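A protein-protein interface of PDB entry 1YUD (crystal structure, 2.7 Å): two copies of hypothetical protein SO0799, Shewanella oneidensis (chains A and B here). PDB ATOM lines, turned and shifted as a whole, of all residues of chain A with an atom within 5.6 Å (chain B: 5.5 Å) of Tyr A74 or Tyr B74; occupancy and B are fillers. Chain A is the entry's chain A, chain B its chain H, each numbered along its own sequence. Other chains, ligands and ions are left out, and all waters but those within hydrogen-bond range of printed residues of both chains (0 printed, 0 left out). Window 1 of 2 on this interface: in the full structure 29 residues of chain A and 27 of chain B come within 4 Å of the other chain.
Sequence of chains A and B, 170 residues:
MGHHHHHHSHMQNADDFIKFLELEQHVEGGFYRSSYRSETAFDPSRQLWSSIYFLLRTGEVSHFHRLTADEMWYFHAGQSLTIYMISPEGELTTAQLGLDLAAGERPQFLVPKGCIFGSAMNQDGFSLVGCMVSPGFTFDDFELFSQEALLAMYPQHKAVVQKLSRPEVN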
ATOM      1  N   TRP A  49     -20.169  12.786  -5.288  1.00  0.00           N
ATOM      2  CA  TRP A  49     -20.848  14.078  -5.400  1.00  0.00           C
ATOM      3  C   TRP A  49     -22.377  13.989  -5.514  1.00  0.00           C
ATOM      4  O   TRP A  49     -22.955  12.903  -5.576  1.00  0.00           O
ATOM      5  CB  TRP A  49     -20.292  14.890  -6.575  1.00  0.00           C
ATOM      6  CG  TRP A  49     -20.474  14.288  -7.944  1.00  0.00           C
ATOM      7  CD1 TRP A  49     -19.543  13.605  -8.665  1.00  0.00           C
ATOM      8  CD2 TRP A  49     -21.651  14.341  -8.761  1.00  0.00           C
ATOM      9  NE1 TRP A  49     -20.058  13.232  -9.881  1.00  0.00           N
ATOM     10  CE2 TRP A  49     -21.354  13.668  -9.969  1.00  0.00           C
ATOM     11  CE3 TRP A  49     -22.932  14.892  -8.592  1.00  0.00           C
ATOM     12  CZ2 TRP A  49     -22.283  13.527 -11.003  1.00  0.00           C
ATOM     13  CZ3 TRP A  49     -23.860  14.755  -9.622  1.00  0.00           C
ATOM     14  CH2 TRP A  49     -23.527  14.074 -10.814  1.00  0.00           C
ATOM     15  N   SER A  50     -23.019  15.152  -5.530  1.00  0.00           N
ATOM     16  CA  SER A  50     -24.472  15.255  -5.627  1.00  0.00           C
ATOM     17  C   SER A  50     -24.906  16.662  -6.057  1.00  0.00           C
ATOM     18  O   SER A  50     -24.287  17.652  -5.685  1.00  0.00           O
ATOM     19  CB  SER A  50     -25.104  14.923  -4.272  1.00  0.00           C
ATOM     20  OG  SER A  50     -24.621  15.765  -3.244  1.00  0.00           O
ATOM     21  N   SER A  51     -25.963  16.750  -6.852  1.00  0.00           N
ATOM     22  CA  SER A  51     -26.475  18.044  -7.286  1.00  0.00           C
ATOM     23  C   SER A  51     -27.984  18.074  -7.069  1.00  0.00           C
ATOM     24  O   SER A  51     -28.658  17.059  -7.199  1.00  0.00           O
ATOM     25  CB  SER A  51     -26.181  18.280  -8.767  1.00  0.00           C
ATOM     26  OG  SER A  51     -26.905  19.401  -9.256  1.00  0.00           O
ATOM     27  N   MET A  72     -20.782  23.958  -4.540  1.00  0.00           N
ATOM     28  CA  MET A  72     -20.672  24.884  -5.627  1.00  0.00           C
ATOM     29  C   MET A  72     -22.067  25.421  -5.914  1.00  0.00           C
ATOM     30  O   MET A  72     -23.069  24.742  -5.692  1.00  0.00           O
ATOM     31  CB  MET A  72     -20.052  24.194  -6.844  1.00  0.00           C
ATOM     32  CG  MET A  72     -18.511  24.178  -6.808  1.00  0.00           C
ATOM     33  SD  MET A  72     -17.708  25.952  -6.993  1.00  0.00           S
ATOM     34  CE  MET A  72     -18.291  26.321  -8.804  1.00  0.00           C
ATOM     35  N   TRP A  73     -22.138  26.661  -6.369  1.00  0.00           N
ATOM     36  CA  TRP A  73     -23.415  27.258  -6.674  1.00  0.00           C
ATOM     37  C   TRP A  73     -23.432  27.714  -8.112  1.00  0.00           C
ATOM     38  O   TRP A  73     -22.583  28.493  -8.535  1.00  0.00           O
ATOM     39  CB  TRP A  73     -23.681  28.444  -5.747  1.00  0.00           C
ATOM     40  CG  TRP A  73     -24.140  28.042  -4.368  1.00  0.00           C
ATOM     41  CD1 TRP A  73     -23.491  27.215  -3.497  1.00  0.00           C
ATOM     42  CD2 TRP A  73     -25.337  28.472  -3.696  1.00  0.00           C
ATOM     43  NE1 TRP A  73     -24.206  27.104  -2.323  1.00  0.00           N
ATOM     44  CE2 TRP A  73     -25.344  27.866  -2.419  1.00  0.00           C
ATOM     45  CE3 TRP A  73     -26.403  29.314  -4.051  1.00  0.00           C
ATOM     46  CZ2 TRP A  73     -26.372  28.075  -1.491  1.00  0.00           C
ATOM     47  CZ3 TRP A  73     -27.425  29.524  -3.129  1.00  0.00           C
ATOM     48  CH2 TRP A  73     -27.400  28.904  -1.861  1.00  0.00           C
ATOM     49  N   TYR A  74     -24.399  27.223  -8.873  1.00  0.00           N
ATOM     50  CA  TYR A  74     -24.516  27.617 -10.268  1.00  0.00           C
ATOM     51  C   TYR A  74     -25.764  28.482 -10.365  1.00  0.00           C
ATOM     52  O   TYR A  74     -26.629  28.428  -9.492  1.00  0.00           O
ATOM     53  CB  TYR A  74     -24.624  26.361 -11.139  1.00  0.00           C
ATOM     54  CG  TYR A  74     -23.398  25.483 -11.006  1.00  0.00           C
ATOM     55  CD1 TYR A  74     -22.283  25.688 -11.814  1.00  0.00           C
ATOM     56  CD2 TYR A  74     -23.315  24.525 -10.004  1.00  0.00           C
ATOM     57  CE1 TYR A  74     -21.117  24.967 -11.621  1.00  0.00           C
ATOM     58  CE2 TYR A  74     -22.151  23.807  -9.796  1.00  0.00           C
ATOM     59  CZ  TYR A  74     -21.052  24.039 -10.606  1.00  0.00           C
ATOM     60  OH  TYR A  74     -19.858  23.403 -10.348  1.00  0.00           O
ATOM     61  N   PHE A  75     -25.865  29.286 -11.408  1.00  0.00           N
ATOM     62  CA  PHE A  75     -27.026  30.142 -11.558  1.00  0.00           C
ATOM     63  C   PHE A  75     -27.776  29.807 -12.839  1.00  0.00           C
ATOM     64  O   PHE A  75     -27.237  29.948 -13.947  1.00  0.00           O
ATOM     65  CB  PHE A  75     -26.598  31.610 -11.593  1.00  0.00           C
ATOM     66  CG  PHE A  75     -27.742  32.566 -11.596  1.00  0.00           C
ATOM     67  CD1 PHE A  75     -28.370  32.918 -10.401  1.00  0.00           C
ATOM     68  CD2 PHE A  75     -28.218  33.097 -12.792  1.00  0.00           C
ATOM     69  CE1 PHE A  75     -29.473  33.799 -10.391  1.00  0.00           C
ATOM     70  CE2 PHE A  75     -29.313  33.970 -12.805  1.00  0.00           C
ATOM     71  CZ  PHE A  75     -29.942  34.324 -11.595  1.00  0.00           C
ATOM     72  N   HIS A  76     -29.028  29.389 -12.693  1.00  0.00           N
ATOM     73  CA  HIS A  76     -29.839  29.045 -13.856  1.00  0.00           C
ATOM     74  C   HIS A  76     -30.660  30.212 -14.371  1.00  0.00           C
ATOM     75  O   HIS A  76     -30.578  30.573 -15.555  1.00  0.00           O
ATOM     76  CB  HIS A  76     -30.767  27.890 -13.523  1.00  0.00           C
ATOM     77  CG  HIS A  76     -30.049  26.647 -13.119  1.00  0.00           C
ATOM     78  ND1 HIS A  76     -29.171  25.997 -13.956  1.00  0.00           N
ATOM     79  CD2 HIS A  76     -30.113  25.905 -11.986  1.00  0.00           C
ATOM     80  CE1 HIS A  76     -28.732  24.901 -13.360  1.00  0.00           C
ATOM     81  NE2 HIS A  76     -29.289  24.820 -12.166  1.00  0.00           N
ATOM     82  N   LEU A  97     -24.228  36.254  -6.422  1.00  0.00           N
ATOM     83  CA  LEU A  97     -24.503  35.249  -7.447  1.00  0.00           C
ATOM     84  C   LEU A  97     -25.491  35.879  -8.412  1.00  0.00           C
ATOM     85  O   LEU A  97     -26.335  36.653  -7.982  1.00  0.00           O
ATOM     86  CB  LEU A  97     -25.118  33.997  -6.817  1.00  0.00           C
ATOM     87  CG  LEU A  97     -24.819  32.678  -7.532  1.00  0.00           C
ATOM     88  CD1 LEU A  97     -23.290  32.468  -7.615  1.00  0.00           C
ATOM     89  CD2 LEU A  97     -25.490  31.526  -6.779  1.00  0.00           C
ATOM     90  N   PRO A 107     -21.884  34.066 -12.073  1.00  0.00           N
ATOM     91  CA  PRO A 107     -22.721  32.865 -12.158  1.00  0.00           C
ATOM     92  C   PRO A 107     -22.363  31.706 -11.230  1.00  0.00           C
ATOM     93  O   PRO A 107     -23.232  30.900 -10.882  1.00  0.00           O
ATOM     94  CB  PRO A 107     -22.629  32.489 -13.628  1.00  0.00           C
ATOM     95  CG  PRO A 107     -22.528  33.821 -14.279  1.00  0.00           C
ATOM     96  CD  PRO A 107     -21.489  34.502 -13.419  1.00  0.00           C
ATOM     97  N   GLN A 108     -21.105  31.611 -10.818  1.00  0.00           N
ATOM     98  CA  GLN A 108     -20.722  30.526  -9.916  1.00  0.00           C
ATOM     99  C   GLN A 108     -20.098  31.041  -8.639  1.00  0.00           C
ATOM    100  O   GLN A 108     -19.469  32.090  -8.614  1.00  0.00           O
ATOM    101  CB  GLN A 108     -19.719  29.570 -10.580  1.00  0.00           C
ATOM    102  CG  GLN A 108     -20.334  28.388 -11.315  1.00  0.00           C
ATOM    103  CD  GLN A 108     -19.368  27.771 -12.313  1.00  0.00           C
ATOM    104  OE1 GLN A 108     -18.483  26.982 -11.948  1.00  0.00           O
ATOM    105  NE2 GLN A 108     -19.519  28.145 -13.587  1.00  0.00           N
ATOM    106  N   PHE A 109     -20.273  30.299  -7.567  1.00  0.00           N
ATOM    107  CA  PHE A 109     -19.666  30.698  -6.339  1.00  0.00           C
ATOM    108  C   PHE A 109     -19.424  29.469  -5.501  1.00  0.00           C
ATOM    109  O   PHE A 109     -20.192  28.509  -5.550  1.00  0.00           O
ATOM    110  CB  PHE A 109     -20.526  31.685  -5.565  1.00  0.00           C
ATOM    111  CG  PHE A 109     -19.829  32.220  -4.362  1.00  0.00           C
ATOM    112  CD1 PHE A 109     -18.980  33.310  -4.467  1.00  0.00           C
ATOM    113  CD2 PHE A 109     -19.895  31.547  -3.160  1.00  0.00           C
ATOM    114  CE1 PHE A 109     -18.201  33.711  -3.396  1.00  0.00           C
ATOM    115  CE2 PHE A 109     -19.115  31.948  -2.086  1.00  0.00           C
ATOM    116  CZ  PHE A 109     -18.274  33.026  -2.216  1.00  0.00           C
ATOM    117  N   LEU A 128     -33.901  30.063  -9.415  1.00  0.00           N
ATOM    118  CA  LEU A 128     -33.554  28.665  -9.605  1.00  0.00           C
ATOM    119  C   LEU A 128     -32.034  28.663  -9.483  1.00  0.00           C
ATOM    120  O   LEU A 128     -31.347  29.513 -10.062  1.00  0.00           O
ATOM    121  CB  LEU A 128     -33.968  28.178 -10.997  1.00  0.00           C
ATOM    122  CG  LEU A 128     -33.642  26.691 -11.178  1.00  0.00           C
ATOM    123  CD1 LEU A 128     -34.495  25.898 -10.220  1.00  0.00           C
ATOM    124  CD2 LEU A 128     -33.876  26.240 -12.610  1.00  0.00           C
ATOM    125  N   VAL A 129     -31.517  27.693  -8.744  1.00  0.00           N
ATOM    126  CA  VAL A 129     -30.095  27.616  -8.488  1.00  0.00           C
ATOM    127  C   VAL A 129     -29.579  26.183  -8.467  1.00  0.00           C
ATOM    128  O   VAL A 129     -30.287  25.255  -8.061  1.00  0.00           O
ATOM    129  CB  VAL A 129     -29.800  28.298  -7.134  1.00  0.00           C
ATOM    130  CG1 VAL A 129     -28.928  27.429  -6.254  1.00  0.00           C
ATOM    131  CG2 VAL A 129     -29.196  29.648  -7.376  1.00  0.00           C
ATOM    132  N   GLY A 130     -28.334  26.009  -8.905  1.00  0.00           N
ATOM    133  CA  GLY A 130     -27.741  24.687  -8.893  1.00  0.00           C
ATOM    134  C   GLY A 130     -26.776  24.582  -7.733  1.00  0.00           C
ATOM    135  O   GLY A 130     -25.934  25.457  -7.546  1.00  0.00           O
ATOM    136  N   CYS A 131     -26.900  23.526  -6.944  1.00  0.00           N
ATOM    137  CA  CYS A 131     -26.012  23.329  -5.816  1.00  0.00           C
ATOM    138  C   CYS A 131     -25.376  21.947  -5.852  1.00  0.00           C
ATOM    139  O   CYS A 131     -26.052  20.919  -5.836  1.00  0.00           O
ATOM    140  CB  CYS A 131     -26.758  23.546  -4.494  1.00  0.00           C
ATOM    141  SG  CYS A 131     -27.128  25.295  -4.132  1.00  0.00           S
ATOM    142  N   MET A 132     -24.050  21.956  -5.892  1.00  0.00           N
ATOM    143  CA  MET A 132     -23.236  20.751  -5.955  1.00  0.00           C
ATOM    144  C   MET A 132     -22.305  20.685  -4.745  1.00  0.00           C
ATOM    145  O   MET A 132     -21.386  21.491  -4.630  1.00  0.00           O
ATOM    146  CB  MET A 132     -22.432  20.784  -7.267  1.00  0.00           C
ATOM    147  CG  MET A 132     -21.591  19.553  -7.611  1.00  0.00           C
ATOM    148  SD  MET A 132     -19.929  19.372  -6.614  1.00  0.00           S
ATOM    149  CE  MET A 132     -20.329  17.707  -5.744  1.00  0.00           C
ATOM    150  N   SER B  51     -14.452  22.754 -11.659  1.00  0.00           N
ATOM    151  CA  SER B  51     -15.589  23.454 -12.216  1.00  0.00           C
ATOM    152  C   SER B  51     -15.186  24.643 -13.096  1.00  0.00           C
ATOM    153  O   SER B  51     -14.304  25.433 -12.740  1.00  0.00           O
ATOM    154  CB  SER B  51     -16.478  23.925 -11.071  1.00  0.00           C
ATOM    155  OG  SER B  51     -17.601  24.631 -11.560  1.00  0.00           O
ATOM    156  N   ILE B  52     -15.846  24.779 -14.239  1.00  0.00           N
ATOM    157  CA  ILE B  52     -15.547  25.865 -15.146  1.00  0.00           C
ATOM    158  C   ILE B  52     -16.799  26.573 -15.650  1.00  0.00           C
ATOM    159  O   ILE B  52     -17.907  26.223 -15.267  1.00  0.00           O
ATOM    160  CB  ILE B  52     -14.788  25.367 -16.381  1.00  0.00           C
ATOM    161  CG1 ILE B  52     -15.682  24.430 -17.198  1.00  0.00           C
ATOM    162  CG2 ILE B  52     -13.497  24.680 -15.948  1.00  0.00           C
ATOM    163  CD1 ILE B  52     -15.207  24.219 -18.615  1.00  0.00           C
ATOM    164  N   MET B  72     -21.067  17.133 -14.900  1.00  0.00           N
ATOM    165  CA  MET B  72     -22.306  17.845 -14.590  1.00  0.00           C
ATOM    166  C   MET B  72     -22.444  19.167 -15.366  1.00  0.00           C
ATOM    167  O   MET B  72     -21.558  20.004 -15.333  1.00  0.00           O
ATOM    168  CB  MET B  72     -22.379  18.144 -13.084  1.00  0.00           C
ATOM    169  CG  MET B  72     -22.943  17.012 -12.224  1.00  0.00           C
ATOM    170  SD  MET B  72     -24.755  16.477 -12.761  1.00  0.00           S
ATOM    171  CE  MET B  72     -25.752  18.034 -12.155  1.00  0.00           C
ATOM    172  N   TRP B  73     -23.567  19.342 -16.054  1.00  0.00           N
ATOM    173  CA  TRP B  73     -23.828  20.568 -16.798  1.00  0.00           C
ATOM    174  C   TRP B  73     -24.920  21.447 -16.162  1.00  0.00           C
ATOM    175  O   TRP B  73     -26.046  20.996 -15.966  1.00  0.00           O
ATOM    176  CB  TRP B  73     -24.237  20.238 -18.221  1.00  0.00           C
ATOM    177  CG  TRP B  73     -23.101  19.868 -19.106  1.00  0.00           C
ATOM    178  CD1 TRP B  73     -22.228  18.825 -18.945  1.00  0.00           C
ATOM    179  CD2 TRP B  73     -22.768  20.487 -20.349  1.00  0.00           C
ATOM    180  NE1 TRP B  73     -21.385  18.754 -20.028  1.00  0.00           N
ATOM    181  CE2 TRP B  73     -21.696  19.762 -20.905  1.00  0.00           C
ATOM    182  CE3 TRP B  73     -23.280  21.584 -21.051  1.00  0.00           C
ATOM    183  CZ2 TRP B  73     -21.124  20.092 -22.129  1.00  0.00           C
ATOM    184  CZ3 TRP B  73     -22.716  21.920 -22.276  1.00  0.00           C
ATOM    185  CH2 TRP B  73     -21.646  21.170 -22.805  1.00  0.00           C
ATOM    186  N   TYR B  74     -24.576  22.704 -15.872  1.00  0.00           N
ATOM    187  CA  TYR B  74     -25.491  23.674 -15.268  1.00  0.00           C
ATOM    188  C   TYR B  74     -25.795  24.834 -16.211  1.00  0.00           C
ATOM    189  O   TYR B  74     -24.941  25.682 -16.417  1.00  0.00           O
ATOM    190  CB  TYR B  74     -24.840  24.240 -14.027  1.00  0.00           C
ATOM    191  CG  TYR B  74     -24.537  23.203 -12.994  1.00  0.00           C
ATOM    192  CD1 TYR B  74     -25.492  22.865 -12.035  1.00  0.00           C
ATOM    193  CD2 TYR B  74     -23.312  22.528 -12.986  1.00  0.00           C
ATOM    194  CE1 TYR B  74     -25.248  21.876 -11.091  1.00  0.00           C
ATOM    195  CE2 TYR B  74     -23.051  21.526 -12.039  1.00  0.00           C
ATOM    196  CZ  TYR B  74     -24.036  21.207 -11.097  1.00  0.00           C
ATOM    197  OH  TYR B  74     -23.843  20.213 -10.170  1.00  0.00           O
ATOM    198  N   PHE B  75     -26.990  24.901 -16.784  1.00  0.00           N
ATOM    199  CA  PHE B  75     -27.274  26.027 -17.663  1.00  0.00           C
ATOM    200  C   PHE B  75     -27.229  27.350 -16.908  1.00  0.00           C
ATOM    201  O   PHE B  75     -27.964  27.525 -15.936  1.00  0.00           O
ATOM    202  CB  PHE B  75     -28.643  25.941 -18.288  1.00  0.00           C
ATOM    203  CG  PHE B  75     -28.953  27.107 -19.179  1.00  0.00           C
ATOM    204  CD1 PHE B  75     -28.628  27.062 -20.526  1.00  0.00           C
ATOM    205  CD2 PHE B  75     -29.582  28.253 -18.665  1.00  0.00           C
ATOM    206  CE1 PHE B  75     -28.928  28.138 -21.374  1.00  0.00           C
ATOM    207  CE2 PHE B  75     -29.889  29.344 -19.497  1.00  0.00           C
ATOM    208  CZ  PHE B  75     -29.561  29.280 -20.857  1.00  0.00           C
ATOM    209  N   HIS B  76     -26.395  28.276 -17.402  1.00  0.00           N
ATOM    210  CA  HIS B  76     -26.186  29.603 -16.823  1.00  0.00           C
ATOM    211  C   HIS B  76     -26.914  30.749 -17.523  1.00  0.00           C
ATOM    212  O   HIS B  76     -27.392  31.654 -16.854  1.00  0.00           O
ATOM    213  CB  HIS B  76     -24.695  29.950 -16.822  1.00  0.00           C
ATOM    214  CG  HIS B  76     -23.939  29.418 -15.647  1.00  0.00           C
ATOM    215  ND1 HIS B  76     -24.553  29.053 -14.470  1.00  0.00           N
ATOM    216  CD2 HIS B  76     -22.611  29.242 -15.450  1.00  0.00           C
ATOM    217  CE1 HIS B  76     -23.635  28.675 -13.597  1.00  0.00           C
ATOM    218  NE2 HIS B  76     -22.449  28.780 -14.168  1.00  0.00           N
ATOM    219  N   LEU B  97     -30.283  21.327 -22.859  1.00  0.00           N
ATOM    220  CA  LEU B  97     -30.052  22.027 -21.610  1.00  0.00           C
ATOM    221  C   LEU B  97     -30.635  23.408 -21.781  1.00  0.00           C
ATOM    222  O   LEU B  97     -30.495  24.009 -22.850  1.00  0.00           O
ATOM    223  CB  LEU B  97     -28.556  22.117 -21.344  1.00  0.00           C
ATOM    224  CG  LEU B  97     -28.133  22.488 -19.927  1.00  0.00           C
ATOM    225  CD1 LEU B  97     -28.202  21.248 -19.058  1.00  0.00           C
ATOM    226  CD2 LEU B  97     -26.725  23.064 -19.926  1.00  0.00           C
ATOM    227  N   PRO B 107     -32.518  22.498 -16.876  1.00  0.00           N
ATOM    228  CA  PRO B 107     -31.415  23.424 -16.601  1.00  0.00           C
ATOM    229  C   PRO B 107     -30.130  22.691 -16.214  1.00  0.00           C
ATOM    230  O   PRO B 107     -29.066  23.292 -16.096  1.00  0.00           O
ATOM    231  CB  PRO B 107     -31.952  24.280 -15.448  1.00  0.00           C
ATOM    232  CG  PRO B 107     -33.427  24.095 -15.506  1.00  0.00           C
ATOM    233  CD  PRO B 107     -33.562  22.639 -15.854  1.00  0.00           C
ATOM    234  N   GLN B 108     -30.234  21.389 -16.001  1.00  0.00           N
ATOM    235  CA  GLN B 108     -29.076  20.597 -15.621  1.00  0.00           C
ATOM    236  C   GLN B 108     -29.031  19.300 -16.409  1.00  0.00           C
ATOM    237  O   GLN B 108     -30.032  18.876 -16.989  1.00  0.00           O
ATOM    238  CB  GLN B 108     -29.107  20.295 -14.125  1.00  0.00           C
ATOM    239  CG  GLN B 108     -28.597  21.437 -13.269  1.00  0.00           C
ATOM    240  CD  GLN B 108     -28.664  21.144 -11.783  1.00  0.00           C
ATOM    241  OE1 GLN B 108     -28.282  20.062 -11.327  1.00  0.00           O
ATOM    242  NE2 GLN B 108     -29.140  22.122 -11.015  1.00  0.00           N
ATOM    243  N   PHE B 109     -27.861  18.681 -16.450  1.00  0.00           N
ATOM    244  CA  PHE B 109     -27.703  17.428 -17.162  1.00  0.00           C
ATOM    245  C   PHE B 109     -26.354  16.824 -16.868  1.00  0.00           C
ATOM    246  O   PHE B 109     -25.373  17.534 -16.699  1.00  0.00           O
ATOM    247  CB  PHE B 109     -27.851  17.621 -18.668  1.00  0.00           C
ATOM    248  CG  PHE B 109     -27.913  16.330 -19.421  1.00  0.00           C
ATOM    249  CD1 PHE B 109     -29.018  15.502 -19.305  1.00  0.00           C
ATOM    250  CD2 PHE B 109     -26.827  15.888 -20.166  1.00  0.00           C
ATOM    251  CE1 PHE B 109     -29.034  14.255 -19.907  1.00  0.00           C
ATOM    252  CE2 PHE B 109     -26.845  14.630 -20.777  1.00  0.00           C
ATOM    253  CZ  PHE B 109     -27.950  13.821 -20.638  1.00  0.00           C
ATOM    254  N   LEU B 128     -23.905  30.430 -22.304  1.00  0.00           N
ATOM    255  CA  LEU B 128     -22.963  30.216 -21.215  1.00  0.00           C
ATOM    256  C   LEU B 128     -23.471  29.144 -20.277  1.00  0.00           C
ATOM    257  O   LEU B 128     -24.620  29.189 -19.840  1.00  0.00           O
ATOM    258  CB  LEU B 128     -22.756  31.504 -20.429  1.00  0.00           C
ATOM    259  CG  LEU B 128     -21.902  31.370 -19.168  1.00  0.00           C
ATOM    260  CD1 LEU B 128     -20.438  31.094 -19.541  1.00  0.00           C
ATOM    261  CD2 LEU B 128     -22.028  32.655 -18.360  1.00  0.00           C
ATOM    262  N   VAL B 129     -22.603  28.195 -19.945  1.00  0.00           N
ATOM    263  CA  VAL B 129     -22.967  27.080 -19.084  1.00  0.00           C
ATOM    264  C   VAL B 129     -21.971  26.955 -17.945  1.00  0.00           C
ATOM    265  O   VAL B 129     -21.055  27.754 -17.831  1.00  0.00           O
ATOM    266  CB  VAL B 129     -22.932  25.787 -19.885  1.00  0.00           C
ATOM    267  CG1 VAL B 129     -23.536  24.681 -19.092  1.00  0.00           C
ATOM    268  CG2 VAL B 129     -23.656  25.967 -21.198  1.00  0.00           C
ATOM    269  N   GLY B 130     -22.157  25.962 -17.093  1.00  0.00           N
ATOM    270  CA  GLY B 130     -21.241  25.729 -15.999  1.00  0.00           C
ATOM    271  C   GLY B 130     -20.995  24.228 -16.007  1.00  0.00           C
ATOM    272  O   GLY B 130     -21.958  23.448 -15.950  1.00  0.00           O
ATOM    273  N   CYS B 131     -19.738  23.797 -16.092  1.00  0.00           N
ATOM    274  CA  CYS B 131     -19.453  22.368 -16.118  1.00  0.00           C
ATOM    275  C   CYS B 131     -18.730  21.876 -14.868  1.00  0.00           C
ATOM    276  O   CYS B 131     -17.952  22.599 -14.295  1.00  0.00           O
ATOM    277  CB  CYS B 131     -18.636  22.041 -17.355  1.00  0.00           C
ATOM    278  SG  CYS B 131     -19.547  22.176 -18.905  1.00  0.00           S
ATOM    279  N   MET B 132     -18.990  20.662 -14.420  1.00  0.00           N
ATOM    280  CA  MET B 132     -18.293  20.181 -13.249  1.00  0.00           C
ATOM    281  C   MET B 132     -17.994  18.694 -13.437  1.00  0.00           C
ATOM    282  O   MET B 132     -18.906  17.873 -13.595  1.00  0.00           O
ATOM    283  CB  MET B 132     -19.140  20.452 -11.996  1.00  0.00           C
ATOM    284  CG  MET B 132     -18.573  19.947 -10.677  1.00  0.00           C
ATOM    285  SD  MET B 132     -18.531  18.023 -10.530  1.00  0.00           S
ATOM    286  CE  MET B 132     -18.035  17.809  -8.698  1.00  0.00           C
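Printed residues of chain B that touch a printed residue of chain A: Ser B51, Ile B52, Met B72, Tyr B74, Phe B75, His B76, Pro B107, Gln B108, Gly B130 and Met B132.
Hydrophobic or aromatic side chains of chain A within 4 Å of the printed part of chain B: Trp A49, Met A72, Tyr A74, His A76, Pro A107, Leu A128 and Met A132.
Among the printed residues, 25 pairs touch across the chains.
Among the printed residues, no Asp or Glu carboxylate lies within 4 Å of a Lys or Arg side-chain nitrogen of the other chain.
O of Phe B75 is in hydrogen-bond range of ND1 of His A76 (2.8 Å).
O of Phe A75 sits at hydrogen-bond distance from ND1 of His B76 (2.9 Å).
OG of Ser A51 lies within hydrogen-bond range of OH of Tyr B74 (3.3 Å).
NE2 of Gln A108 sits at hydrogen-bond distance from O of Ile B52, at 3.0 Å.
The backbone carbonyl oxygen (O) of Phe A75 sits close to the backbone carbonyl oxygen (O) of Phe B75.
A ring nitrogen (ND1) of His A76 sits close to the backbone carbonyl oxygen (O) of Pro B107, at 3.5 Å.
The side-chain hydroxyl of Ser A51 is in hydrogen-bond range of the side-chain amide oxygen of Gln B108, 2.6 Å away.
The side-chain hydroxyl (OG) of Ser B51 lies within hydrogen-bond range of the side-chain hydroxyl (OH) of Tyr A74 (2.8 Å).
NE2 of His A76 is in hydrogen-bond range of NE2 of Gln B108, 2.9 Å away.
OE1 of Gln A108 is in hydrogen-bond range of OG of Ser B51.
A ring nitrogen (NE2) of His B76 is in hydrogen-bond range of the side-chain amide nitrogen of Gln A108 (3.1 Å).
Among the printed residues, pairs that only touch across the chains: Met A132 with Met B132 (3.2 Å), Tyr A74 with Tyr B74 (3.2 Å), Met A132 with Tyr B74 (3.3 Å), Met A72 with Ser B51 (3.3 Å), Trp A49 with Met B72 (3.3 Å), Ser A51 with Met B72 (3.4 Å), Tyr A74 with Met B132 (3.5 Å), Tyr A74 with His B76 (3.5 Å), Pro A107 with His B76 (3.5 Å), His A76 with His B76 (3.6 Å), Gly A130 with Gln B108 (3.6 Å), Leu A128 with Pro B107 (3.6 Å), Gln A108 with Gly B130 (3.8 Å) and His A76 with Tyr B74 (3.96 Å).
Printed residues of chain B within 4 Å of Trp A49: Met B72 (3.3 Å).
Of chain B, only Ser B51 (2.8 Å), Tyr B74 (3.2 Å), His B76 (3.5 Å) and Met B132 (3.5 Å) come within 4 Å of Tyr A74.
Tyr B74 touches just these residues of chain A: Ser A51 (3.3 Å), Tyr A74 (3.2 Å), His A76 (3.96 Å) and Met A132 (3.3 Å).
Printed residues of chain A within 4 Å of Met B132: Tyr A74 (3.5 Å) and Met A132 (3.2 Å).
The nearest residue of chain B that does not touch Tyr A74 is Gly B130 (4.3 Å).
The nearest printed residue of chain B that does not touch Pro A107 is Leu B128 (4.3 Å).
Ser A51 touches Gln B108, and with the chains exchanged Gln A108 touches Ser B51.
Tyr B74 touches its own counterpart, Tyr A74.
Phe B75 touches its own counterpart, Phe A75.
Leu A128 touches Pro B107, but with the chains exchanged Pro A107 does not touch Leu B128 (4.3 Å).
Positions printed for both chains: 51, 72, 73, 74, 75, 76, 97, 107, 108, 109, 128, 129, 130, 131 and 132.
Of the 25 pairs that touch across the chains among the printed residues, 22 have their exchanged pair printed and touching as well.
The backbone NH of Met A72 is in hydrogen-bond range of the backbone carbonyl oxygen of Met A132 (2.5 Å).
The backbone NH (N) of Phe B75 sits at hydrogen-bond distance from the backbone carbonyl oxygen (O) of Pro B107 (2.7 Å).
N of Ile B52 lies within hydrogen-bond range of O of Cys B131 (3.0 Å).
O of Leu B128 sits close to N of His B76, 3.2 Å away.
The backbone NH (N) of Tyr A74 sits at hydrogen-bond distance from the backbone carbonyl oxygen (O) of Gly A130 (2.7 Å).
The backbone carbonyl oxygen (O) of Cys B131 lies close to the side-chain hydroxyl (OG) of Ser B51, at 3.4 Å.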
